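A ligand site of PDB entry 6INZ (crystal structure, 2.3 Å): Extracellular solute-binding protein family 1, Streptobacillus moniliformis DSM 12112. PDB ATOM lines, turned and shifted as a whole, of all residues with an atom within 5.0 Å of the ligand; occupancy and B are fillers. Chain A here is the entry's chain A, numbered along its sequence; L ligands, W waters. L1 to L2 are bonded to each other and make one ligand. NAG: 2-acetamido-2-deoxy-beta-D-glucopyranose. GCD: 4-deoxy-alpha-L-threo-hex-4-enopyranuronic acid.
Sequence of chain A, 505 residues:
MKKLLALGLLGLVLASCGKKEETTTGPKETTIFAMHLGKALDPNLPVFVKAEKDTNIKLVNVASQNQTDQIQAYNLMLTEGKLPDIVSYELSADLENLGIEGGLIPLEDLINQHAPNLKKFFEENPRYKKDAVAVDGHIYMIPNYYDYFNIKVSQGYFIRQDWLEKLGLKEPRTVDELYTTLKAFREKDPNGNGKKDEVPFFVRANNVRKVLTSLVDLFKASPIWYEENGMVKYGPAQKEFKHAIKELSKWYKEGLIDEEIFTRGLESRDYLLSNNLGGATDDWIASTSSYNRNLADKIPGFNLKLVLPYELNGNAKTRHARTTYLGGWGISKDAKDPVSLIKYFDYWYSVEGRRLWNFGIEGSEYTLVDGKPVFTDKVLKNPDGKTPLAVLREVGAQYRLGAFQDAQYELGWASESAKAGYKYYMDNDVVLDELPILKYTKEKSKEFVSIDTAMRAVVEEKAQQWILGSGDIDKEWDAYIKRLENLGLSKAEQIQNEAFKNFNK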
ATOM      1  N   HIS A  36      12.098  -0.104  18.451  1.00  0.00           N
ATOM      2  CA  HIS A  36      13.107   0.164  19.463  1.00  0.00           C
ATOM      3  C   HIS A  36      12.666  -0.404  20.802  1.00  0.00           C
ATOM      4  O   HIS A  36      11.529  -0.154  21.261  1.00  0.00           O
ATOM      5  CB  HIS A  36      13.367   1.649  19.612  1.00  0.00           C
ATOM      6  CG  HIS A  36      14.459   1.979  20.591  1.00  0.00           C
ATOM      7  ND1 HIS A  36      15.700   1.363  20.570  1.00  0.00           N
ATOM      8  CD2 HIS A  36      14.488   2.858  21.621  1.00  0.00           C
ATOM      9  CE1 HIS A  36      16.452   1.843  21.542  1.00  0.00           C
ATOM     10  NE2 HIS A  36      15.732   2.761  22.206  1.00  0.00           N
ATOM     11  N   LEU A  37      13.570  -1.146  21.448  1.00  0.00           N
ATOM     12  CA  LEU A  37      13.243  -1.787  22.722  1.00  0.00           C
ATOM     13  C   LEU A  37      11.939  -2.624  22.627  1.00  0.00           C
ATOM     14  O   LEU A  37      11.055  -2.540  23.478  1.00  0.00           O
ATOM     15  CB  LEU A  37      13.120  -0.734  23.838  1.00  0.00           C
ATOM     16  CG  LEU A  37      14.334   0.122  24.138  1.00  0.00           C
ATOM     17  CD1 LEU A  37      13.980   1.257  25.031  1.00  0.00           C
ATOM     18  CD2 LEU A  37      15.421  -0.768  24.700  1.00  0.00           C
ATOM     19  N   GLU A  90      18.693  -0.948  14.372  1.00  0.00           N
ATOM     20  CA  GLU A  90      19.700  -0.978  15.415  1.00  0.00           C
ATOM     21  C   GLU A  90      21.012  -1.648  14.995  1.00  0.00           C
ATOM     22  O   GLU A  90      22.029  -1.382  15.627  1.00  0.00           O
ATOM     23  CB  GLU A  90      19.145  -1.721  16.622  1.00  0.00           C
ATOM     24  CG  GLU A  90      20.005  -1.608  17.851  1.00  0.00           C
ATOM     25  CD  GLU A  90      19.349  -2.116  19.169  1.00  0.00           C
ATOM     26  OE1 GLU A  90      18.296  -1.535  19.562  1.00  0.00           O
ATOM     27  OE2 GLU A  90      19.926  -3.048  19.789  1.00  0.00           O
ATOM     28  N   ASN A 144      22.276   6.995  15.105  1.00  0.00           N
ATOM     29  CA  ASN A 144      21.731   7.560  16.350  1.00  0.00           C
ATOM     30  C   ASN A 144      22.891   7.695  17.338  1.00  0.00           C
ATOM     31  O   ASN A 144      23.303   6.721  17.966  1.00  0.00           O
ATOM     32  CB  ASN A 144      20.599   6.695  16.917  1.00  0.00           C
ATOM     33  CG  ASN A 144      19.686   7.457  17.855  1.00  0.00           C
ATOM     34  OD1 ASN A 144      18.654   8.035  17.418  1.00  0.00           O
ATOM     35  ND2 ASN A 144      20.071   7.518  19.164  1.00  0.00           N
ATOM     36  N   TYR A 146      24.978   8.696  20.693  1.00  0.00           N
ATOM     37  CA  TYR A 146      25.077   9.094  22.074  1.00  0.00           C
ATOM     38  C   TYR A 146      25.834  10.394  22.198  1.00  0.00           C
ATOM     39  O   TYR A 146      26.567  10.793  21.283  1.00  0.00           O
ATOM     40  CB  TYR A 146      25.831   8.071  22.872  1.00  0.00           C
ATOM     41  CG  TYR A 146      25.085   6.816  23.090  1.00  0.00           C
ATOM     42  CD1 TYR A 146      24.015   6.801  23.996  1.00  0.00           C
ATOM     43  CD2 TYR A 146      25.464   5.602  22.427  1.00  0.00           C
ATOM     44  CE1 TYR A 146      23.309   5.584  24.278  1.00  0.00           C
ATOM     45  CE2 TYR A 146      24.745   4.373  22.667  1.00  0.00           C
ATOM     46  CZ  TYR A 146      23.689   4.398  23.615  1.00  0.00           C
ATOM     47  OH  TYR A 146      22.957   3.295  23.949  1.00  0.00           O
ATOM     48  N   ARG A 204      18.191  -6.575  33.351  1.00  0.00           N
ATOM     49  CA  ARG A 204      17.088  -6.031  32.547  1.00  0.00           C
ATOM     50  C   ARG A 204      17.403  -6.203  31.058  1.00  0.00           C
ATOM     51  O   ARG A 204      18.356  -5.608  30.553  1.00  0.00           O
ATOM     52  CB  ARG A 204      16.874  -4.567  32.898  1.00  0.00           C
ATOM     53  CG  ARG A 204      15.768  -3.889  32.128  1.00  0.00           C
ATOM     54  CD  ARG A 204      15.541  -2.511  32.755  1.00  0.00           C
ATOM     55  NE  ARG A 204      16.725  -1.696  32.591  1.00  0.00           N
ATOM     56  CZ  ARG A 204      16.910  -0.782  31.647  1.00  0.00           C
ATOM     57  NH1 ARG A 204      15.935  -0.503  30.743  1.00  0.00           N
ATOM     58  NH2 ARG A 204      18.093  -0.099  31.630  1.00  0.00           N
ATOM     59  N   LYS A 210      21.334  -9.390  25.434  1.00  0.00           N
ATOM     60  CA  LYS A 210      21.347  -8.442  26.555  1.00  0.00           C
ATOM     61  C   LYS A 210      21.423  -9.162  27.912  1.00  0.00           C
ATOM     62  O   LYS A 210      22.057  -8.641  28.858  1.00  0.00           O
ATOM     63  CB  LYS A 210      20.133  -7.493  26.508  1.00  0.00           C
ATOM     64  CG  LYS A 210      20.208  -6.441  25.390  1.00  0.00           C
ATOM     65  CD  LYS A 210      19.051  -5.383  25.420  1.00  0.00           C
ATOM     66  CE  LYS A 210      19.446  -4.334  24.393  1.00  0.00           C
ATOM     67  NZ  LYS A 210      18.846  -2.982  24.606  1.00  0.00           N
ATOM     68  N   LEU A 266      11.839  -6.206  29.593  1.00  0.00           N
ATOM     69  CA  LEU A 266      12.426  -4.968  30.126  1.00  0.00           C
ATOM     70  C   LEU A 266      11.768  -4.491  31.423  1.00  0.00           C
ATOM     71  O   LEU A 266      12.257  -3.542  32.062  1.00  0.00           O
ATOM     72  CB  LEU A 266      12.382  -3.862  29.033  1.00  0.00           C
ATOM     73  CG  LEU A 266      13.303  -4.206  27.827  1.00  0.00           C
ATOM     74  CD1 LEU A 266      13.073  -3.285  26.607  1.00  0.00           C
ATOM     75  CD2 LEU A 266      14.803  -4.182  28.251  1.00  0.00           C
ATOM     76  N   ARG A 269      13.418  -5.111  36.037  1.00  0.00           N
ATOM     77  CA  ARG A 269      13.964  -4.248  37.078  1.00  0.00           C
ATOM     78  C   ARG A 269      12.847  -3.621  37.879  1.00  0.00           C
ATOM     79  O   ARG A 269      12.820  -3.653  39.130  1.00  0.00           O
ATOM     80  CB  ARG A 269      14.833  -3.150  36.472  1.00  0.00           C
ATOM     81  CG  ARG A 269      15.482  -2.262  37.470  1.00  0.00           C
ATOM     82  CD  ARG A 269      16.302  -1.168  36.851  1.00  0.00           C
ATOM     83  NE  ARG A 269      15.634  -0.424  35.809  1.00  0.00           N
ATOM     84  CZ  ARG A 269      16.249   0.451  35.010  1.00  0.00           C
ATOM     85  NH1 ARG A 269      17.564   0.691  35.148  1.00  0.00           N
ATOM     86  NH2 ARG A 269      15.549   1.129  34.095  1.00  0.00           N
ATOM     87  N   TRP A 284      22.241   0.338  33.742  1.00  0.00           N
ATOM     88  CA  TRP A 284      22.548   1.744  33.411  1.00  0.00           C
ATOM     89  C   TRP A 284      22.494   2.620  34.656  1.00  0.00           C
ATOM     90  O   TRP A 284      21.543   2.533  35.427  1.00  0.00           O
ATOM     91  CB  TRP A 284      21.544   2.276  32.372  1.00  0.00           C
ATOM     92  CG  TRP A 284      21.830   1.755  30.971  1.00  0.00           C
ATOM     93  CD1 TRP A 284      21.620   0.442  30.479  1.00  0.00           C
ATOM     94  CD2 TRP A 284      22.475   2.475  29.909  1.00  0.00           C
ATOM     95  NE1 TRP A 284      22.085   0.357  29.172  1.00  0.00           N
ATOM     96  CE2 TRP A 284      22.618   1.562  28.799  1.00  0.00           C
ATOM     97  CE3 TRP A 284      22.984   3.801  29.799  1.00  0.00           C
ATOM     98  CZ2 TRP A 284      23.178   1.944  27.582  1.00  0.00           C
ATOM     99  CZ3 TRP A 284      23.558   4.182  28.583  1.00  0.00           C
ATOM    100  CH2 TRP A 284      23.657   3.242  27.479  1.00  0.00           C
ATOM    101  N   ILE A 285      23.522   3.452  34.844  1.00  0.00           N
ATOM    102  CA  ILE A 285      23.705   4.125  36.117  1.00  0.00           C
ATOM    103  C   ILE A 285      22.540   5.062  36.414  1.00  0.00           C
ATOM    104  O   ILE A 285      21.924   4.949  37.485  1.00  0.00           O
ATOM    105  CB  ILE A 285      25.063   4.848  36.152  1.00  0.00           C
ATOM    106  CG1 ILE A 285      26.139   3.775  36.277  1.00  0.00           C
ATOM    107  CG2 ILE A 285      25.067   5.951  37.317  1.00  0.00           C
ATOM    108  CD1 ILE A 285      27.575   4.294  36.160  1.00  0.00           C
ATOM    109  N   ALA A 286      22.171   5.958  35.475  1.00  0.00           N
ATOM    110  CA  ALA A 286      21.165   6.985  35.804  1.00  0.00           C
ATOM    111  C   ALA A 286      19.803   6.378  36.153  1.00  0.00           C
ATOM    112  O   ALA A 286      19.229   6.668  37.199  1.00  0.00           O
ATOM    113  CB  ALA A 286      21.035   8.026  34.664  1.00  0.00           C
ATOM    114  N   SER A 287      19.247   5.539  35.293  1.00  0.00           N
ATOM    115  CA  SER A 287      17.921   5.002  35.577  1.00  0.00           C
ATOM    116  C   SER A 287      17.910   4.051  36.781  1.00  0.00           C
ATOM    117  O   SER A 287      16.919   3.981  37.510  1.00  0.00           O
ATOM    118  CB  SER A 287      17.395   4.301  34.341  1.00  0.00           C
ATOM    119  OG  SER A 287      18.288   3.186  34.053  1.00  0.00           O
ATOM    120  N   ARG A 322      29.451   3.272  26.683  1.00  0.00           N
ATOM    121  CA  ARG A 322      28.668   3.678  25.524  1.00  0.00           C
ATOM    122  C   ARG A 322      29.490   3.526  24.228  1.00  0.00           C
ATOM    123  O   ARG A 322      30.722   3.632  24.236  1.00  0.00           O
ATOM    124  CB  ARG A 322      28.195   5.132  25.688  1.00  0.00           C
ATOM    125  CG  ARG A 322      26.925   5.294  26.427  1.00  0.00           C
ATOM    126  CD  ARG A 322      26.682   6.759  26.795  1.00  0.00           C
ATOM    127  NE  ARG A 322      26.181   6.773  28.168  1.00  0.00           N
ATOM    128  CZ  ARG A 322      25.103   7.440  28.582  1.00  0.00           C
ATOM    129  NH1 ARG A 322      24.374   8.256  27.789  1.00  0.00           N
ATOM    130  NH2 ARG A 322      24.801   7.321  29.853  1.00  0.00           N
ATOM    131  N   LEU A 326      24.399   4.101  18.178  1.00  0.00           N
ATOM    132  CA  LEU A 326      23.642   2.859  18.235  1.00  0.00           C
ATOM    133  C   LEU A 326      22.663   2.884  17.083  1.00  0.00           C
ATOM    134  O   LEU A 326      21.680   3.628  17.155  1.00  0.00           O
ATOM    135  CB  LEU A 326      22.882   2.731  19.558  1.00  0.00           C
ATOM    136  CG  LEU A 326      22.022   1.478  19.659  1.00  0.00           C
ATOM    137  CD1 LEU A 326      22.922   0.200  19.597  1.00  0.00           C
ATOM    138  CD2 LEU A 326      21.162   1.527  20.910  1.00  0.00           C
ATOM    139  N   LEU A 389      13.196   8.265  32.655  1.00  0.00           N
ATOM    140  CA  LEU A 389      13.408   7.854  31.272  1.00  0.00           C
ATOM    141  C   LEU A 389      12.162   7.178  30.715  1.00  0.00           C
ATOM    142  O   LEU A 389      11.788   7.402  29.556  1.00  0.00           O
ATOM    143  CB  LEU A 389      14.609   6.902  31.198  1.00  0.00           C
ATOM    144  CG  LEU A 389      14.892   6.352  29.827  1.00  0.00           C
ATOM    145  CD1 LEU A 389      14.901   7.482  28.808  1.00  0.00           C
ATOM    146  CD2 LEU A 389      16.294   5.721  29.824  1.00  0.00           C
ATOM    147  N   ARG A 393      10.062   8.021  27.493  1.00  0.00           N
ATOM    148  CA  ARG A 393       9.851   7.162  26.323  1.00  0.00           C
ATOM    149  C   ARG A 393       8.362   7.043  25.987  1.00  0.00           C
ATOM    150  O   ARG A 393       7.985   6.871  24.796  1.00  0.00           O
ATOM    151  CB  ARG A 393      10.454   5.769  26.509  1.00  0.00           C
ATOM    152  CG  ARG A 393      11.952   5.768  26.592  1.00  0.00           C
ATOM    153  CD  ARG A 393      12.435   4.339  26.519  1.00  0.00           C
ATOM    154  NE  ARG A 393      13.882   4.309  26.718  1.00  0.00           N
ATOM    155  CZ  ARG A 393      14.756   4.632  25.769  1.00  0.00           C
ATOM    156  NH1 ARG A 393      14.317   5.038  24.551  1.00  0.00           N
ATOM    157  NH2 ARG A 393      16.055   4.592  26.068  1.00  0.00           N
ATOM    158  N   GLN A 398      13.492  10.116  23.065  1.00  0.00           N
ATOM    159  CA  GLN A 398      14.614   9.150  23.105  1.00  0.00           C
ATOM    160  C   GLN A 398      14.373   7.921  22.243  1.00  0.00           C
ATOM    161  O   GLN A 398      15.035   6.879  22.444  1.00  0.00           O
ATOM    162  CB  GLN A 398      14.926   8.729  24.546  1.00  0.00           C
ATOM    163  CG  GLN A 398      15.288   9.866  25.443  1.00  0.00           C
ATOM    164  CD  GLN A 398      16.599  10.441  25.079  1.00  0.00           C
ATOM    165  OE1 GLN A 398      17.538   9.689  24.674  1.00  0.00           O
ATOM    166  NE2 GLN A 398      16.753  11.789  25.238  1.00  0.00           N
ATOM    167  N   ARG A 400      15.013   5.630  19.449  1.00  0.00           N
ATOM    168  CA  ARG A 400      16.237   5.464  18.667  1.00  0.00           C
ATOM    169  C   ARG A 400      15.932   5.526  17.187  1.00  0.00           C
ATOM    170  O   ARG A 400      15.165   4.692  16.655  1.00  0.00           O
ATOM    171  CB  ARG A 400      16.894   4.112  19.049  1.00  0.00           C
ATOM    172  CG  ARG A 400      18.431   3.932  18.708  1.00  0.00           C
ATOM    173  CD  ARG A 400      18.693   3.484  17.287  1.00  0.00           C
ATOM    174  NE  ARG A 400      17.838   2.397  16.852  1.00  0.00           N
ATOM    175  CZ  ARG A 400      17.356   2.331  15.608  1.00  0.00           C
ATOM    176  NH1 ARG A 400      17.704   3.272  14.705  1.00  0.00           N
ATOM    177  NH2 ARG A 400      16.521   1.360  15.288  1.00  0.00           N
ATOM    178  N   GLN A 405      21.657  12.448  20.638  1.00  0.00           N
ATOM    179  CA  GLN A 405      21.344  12.566  22.045  1.00  0.00           C
ATOM    180  C   GLN A 405      22.119  13.721  22.688  1.00  0.00           C
ATOM    181  O   GLN A 405      23.268  13.999  22.316  1.00  0.00           O
ATOM    182  CB  GLN A 405      21.693  11.294  22.772  1.00  0.00           C
ATOM    183  CG  GLN A 405      21.257  11.289  24.238  1.00  0.00           C
ATOM    184  CD  GLN A 405      21.584   9.969  24.961  1.00  0.00           C
ATOM    185  OE1 GLN A 405      22.725   9.706  25.355  1.00  0.00           O
ATOM    186  NE2 GLN A 405      20.600   9.118  25.076  1.00  0.00           N
ATOM    187  N   TYR A 409      19.896  16.318  28.581  1.00  0.00           N
ATOM    188  CA  TYR A 409      18.665  15.627  28.916  1.00  0.00           C
ATOM    189  C   TYR A 409      18.926  14.610  30.025  1.00  0.00           C
ATOM    190  O   TYR A 409      18.126  14.461  30.944  1.00  0.00           O
ATOM    191  CB  TYR A 409      18.078  14.965  27.668  1.00  0.00           C
ATOM    192  CG  TYR A 409      17.996  13.434  27.809  1.00  0.00           C
ATOM    193  CD1 TYR A 409      19.099  12.616  27.452  1.00  0.00           C
ATOM    194  CD2 TYR A 409      16.851  12.812  28.311  1.00  0.00           C
ATOM    195  CE1 TYR A 409      19.060  11.260  27.620  1.00  0.00           C
ATOM    196  CE2 TYR A 409      16.794  11.424  28.398  1.00  0.00           C
ATOM    197  CZ  TYR A 409      17.919  10.667  28.074  1.00  0.00           C
ATOM    198  OH  TYR A 409      17.902   9.276  28.193  1.00  0.00           O
ATOM    199  N   GLU A 410      20.038  13.916  29.963  1.00  0.00           N
ATOM    200  CA  GLU A 410      20.306  12.874  30.941  1.00  0.00           C
ATOM    201  C   GLU A 410      20.702  13.500  32.277  1.00  0.00           C
ATOM    202  O   GLU A 410      20.228  13.084  33.338  1.00  0.00           O
ATOM    203  CB  GLU A 410      21.407  11.955  30.411  1.00  0.00           C
ATOM    204  CG  GLU A 410      21.504  10.686  31.222  1.00  0.00           C
ATOM    205  CD  GLU A 410      22.483   9.655  30.620  1.00  0.00           C
ATOM    206  OE1 GLU A 410      22.782   9.703  29.357  1.00  0.00           O
ATOM    207  OE2 GLU A 410      22.975   8.840  31.469  1.00  0.00           O
ATOM    208  N   TRP A 413      17.553  14.723  34.424  1.00  0.00           N
ATOM    209  CA  TRP A 413      16.784  13.913  35.376  1.00  0.00           C
ATOM    210  C   TRP A 413      17.638  13.024  36.274  1.00  0.00           C
ATOM    211  O   TRP A 413      17.121  12.485  37.249  1.00  0.00           O
ATOM    212  CB  TRP A 413      15.758  13.028  34.635  1.00  0.00           C
ATOM    213  CG  TRP A 413      16.315  12.101  33.600  1.00  0.00           C
ATOM    214  CD1 TRP A 413      16.450  12.364  32.263  1.00  0.00           C
ATOM    215  CD2 TRP A 413      16.828  10.761  33.793  1.00  0.00           C
ATOM    216  NE1 TRP A 413      16.969  11.249  31.601  1.00  0.00           N
ATOM    217  CE2 TRP A 413      17.221  10.260  32.519  1.00  0.00           C
ATOM    218  CE3 TRP A 413      16.941   9.920  34.908  1.00  0.00           C
ATOM    219  CZ2 TRP A 413      17.780   8.951  32.325  1.00  0.00           C
ATOM    220  CZ3 TRP A 413      17.507   8.604  34.714  1.00  0.00           C
ATOM    221  CH2 TRP A 413      17.902   8.145  33.432  1.00  0.00           C
HETATM  222  C1  NAG L   1      19.608   0.910  24.926  1.00  0.00           C
HETATM  223  C2  NAG L   1      19.108   2.356  25.178  1.00  0.00           C
HETATM  224  C3  NAG L   1      19.355   2.687  26.637  1.00  0.00           C
HETATM  225  C4  NAG L   1      18.601   1.632  27.502  1.00  0.00           C
HETATM  226  C5  NAG L   1      18.932   0.178  27.089  1.00  0.00           C
HETATM  227  C6  NAG L   1      18.156  -0.914  27.811  1.00  0.00           C
HETATM  228  C7  NAG L   1      19.248   4.019  23.471  1.00  0.00           C
HETATM  229  C8  NAG L   1      20.129   4.795  22.526  1.00  0.00           C
HETATM  230  N2  NAG L   1      19.866   3.253  24.369  1.00  0.00           N
HETATM  231  O1  NAG L   1      19.180   0.661  23.590  1.00  0.00           O
HETATM  232  O3  NAG L   1      18.977   4.068  26.954  1.00  0.00           O
HETATM  233  O4  NAG L   1      18.899   1.792  28.918  1.00  0.00           O
HETATM  234  O5  NAG L   1      18.843  -0.063  25.663  1.00  0.00           O
HETATM  235  O6  NAG L   1      18.621  -2.077  27.174  1.00  0.00           O
HETATM  236  O7  NAG L   1      18.002   4.075  23.477  1.00  0.00           O
HETATM  237  C1  GCD L   2      19.816   4.722  27.897  1.00  0.00           C
HETATM  238  C2  GCD L   2      19.745   6.161  27.514  1.00  0.00           C
HETATM  239  C3  GCD L   2      20.719   6.923  28.438  1.00  0.00           C
HETATM  240  C4  GCD L   2      20.438   6.585  29.884  1.00  0.00           C
HETATM  241  C5  GCD L   2      19.860   5.418  30.205  1.00  0.00           C
HETATM  242  C6  GCD L   2      19.660   4.895  31.571  1.00  0.00           C
HETATM  243  O2  GCD L   2      20.162   6.207  26.157  1.00  0.00           O
HETATM  244  O3  GCD L   2      20.432   8.321  28.300  1.00  0.00           O
HETATM  245  O5  GCD L   2      19.312   4.569  29.205  1.00  0.00           O
HETATM  246  O6A GCD L   2      20.190   5.404  32.611  1.00  0.00           O
HETATM  247  O6B GCD L   2      18.951   3.886  31.598  1.00  0.00           O
HETATM  248  O   HOH W   1      21.374  -2.055  27.875  1.00  0.00           O
HETATM  249  O   HOH W   2      17.601   6.353  21.694  1.00  0.00           O
HETATM  250  O   HOH W   3      22.777   6.312  32.636  1.00  0.00           O
HETATM  251  O   HOH W   4      19.250  -1.710  22.553  1.00  0.00           O
HETATM  252  O   HOH W   5      22.331   6.286  20.580  1.00  0.00           O
HETATM  253  O   HOH W   6      17.925   7.062  24.521  1.00  0.00           O
HETATM  254  O   HOH W   7      19.123  -3.619  29.275  1.00  0.00           O
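The backbone NH of Ser 287 sits at hydrogen-bond distance from an oxygen (O6A) of GCD L2, 2.8 Å away. The side-chain hydroxyl of Ser 287 is in hydrogen-bond range of an oxygen (O6B) of GCD L2, at 2.6 Å. The side-chain hydroxyl (OH) of Tyr 409 sits at hydrogen-bond distance from an oxygen (O3) of GCD L2 (2.7 Å). An oxygen (O6) of NAG L1 sits at hydrogen-bond distance from the side-chain amino group (NZ) of Lys 210, at 2.7 Å. NE2 of His 36 lies within hydrogen-bond range of O7 of NAG L1, 2.9 Å away. The side-chain carboxylate of Glu 410 sits at hydrogen-bond distance from an oxygen (O3) of GCD L2. NH2 of Arg 393 is in hydrogen-bond range of O3 of NAG L1. OH of Tyr 146 lies within hydrogen-bond range of N2 of NAG L1 (3.1 Å). NE2 of Gln 405 lies within hydrogen-bond range of O2 of GCD L2, 3.1 Å away. O4 of NAG L1 lies within hydrogen-bond range of NH2 of Arg 204 (3.4 Å).
The guanidinium group of Arg 269 sits at hydrogen-bond distance from the side-chain hydroxyl of Ser 287, 2.8 Å away. NE1 of Trp 413 lies close to O of Tyr 409 (3.5 Å). The guanidinium group of Arg 322 lies within salt-bridge range of the side-chain carboxylate of Glu 410 (2.7 Å). The guanidinium group of Arg 393 is in hydrogen-bond range of the backbone carbonyl oxygen of Gln 398 (2.9 Å). OE1 of Gln 405 sits at hydrogen-bond distance from NH1 of Arg 322 (3.3 Å). NE2 of Gln 405 lies within hydrogen-bond range of OE1 of Gln 398 (3.1 Å). The backbone NH of Leu 326 sits at hydrogen-bond distance from the backbone carbonyl oxygen of Asn 144.
Leu 37 touches the ligand. CB of Trp 284 touches O6B of GCD L2, 3.1 Å away. CB of Ala 286 touches O6A of GCD L2 (3.4 Å). Arg 322 touches the ligand. CD2 of Leu 326 touches O1 of NAG L1 (3.4 Å). Leu 389 touches the ligand. CH2 of Trp 413 touches O6A of GCD L2, 3.7 Å away. Hydrophobic or aromatic side chains that line the ligand: His 36, Leu 37, Tyr 146, Trp 284, Ala 286, Leu 326, Leu 389, Tyr 409 and Trp 413. 16 residues have an atom within 4 Å of the ligand: His 36, Leu 37, Tyr 146, Arg 204, Lys 210, Trp 284, Ala 286, Ser 287, Arg 322, Leu 326, Leu 389, Arg 393, Gln 405, Tyr 409, Glu 410 and Trp 413.
Water W4 lies within hydrogen-bond range of the side-chain amino group (NZ) of Lys 210 (2.4 Å), an oxygen (O1) of NAG L1 (2.6 Å) and the side-chain carboxylate (OE1) of Glu 90 (3.1 Å). Water W7 bridges the backbone carbonyl oxygen (O) of Arg 204 (2.5 Å) and an oxygen (O6) of NAG L1 (2.7 Å). Water W3 lies within hydrogen-bond range of an oxygen (O6A) of GCD L2 (2.7 Å), the side-chain carboxylate (OE2) of Glu 410 (2.8 Å) and the backbone NH (N) of Ala 286 (2.9 Å). Water W1 bridges NE1 of Trp 284 (2.8 Å) and O6 of NAG L1 (2.8 Å). Water W6 lies within hydrogen-bond range of the side-chain amide oxygen of Gln 398 (2.7 Å), an oxygen (O2) of GCD L2 (2.9 Å), the side-chain amide nitrogen of Gln 405 (3.4 Å) and the guanidinium group of Arg 393 (3.5 Å). Water W2 lies within hydrogen-bond range of the backbone carbonyl oxygen (O) of Gln 398 (2.7 Å) and an oxygen (O7) of NAG L1 (2.9 Å).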
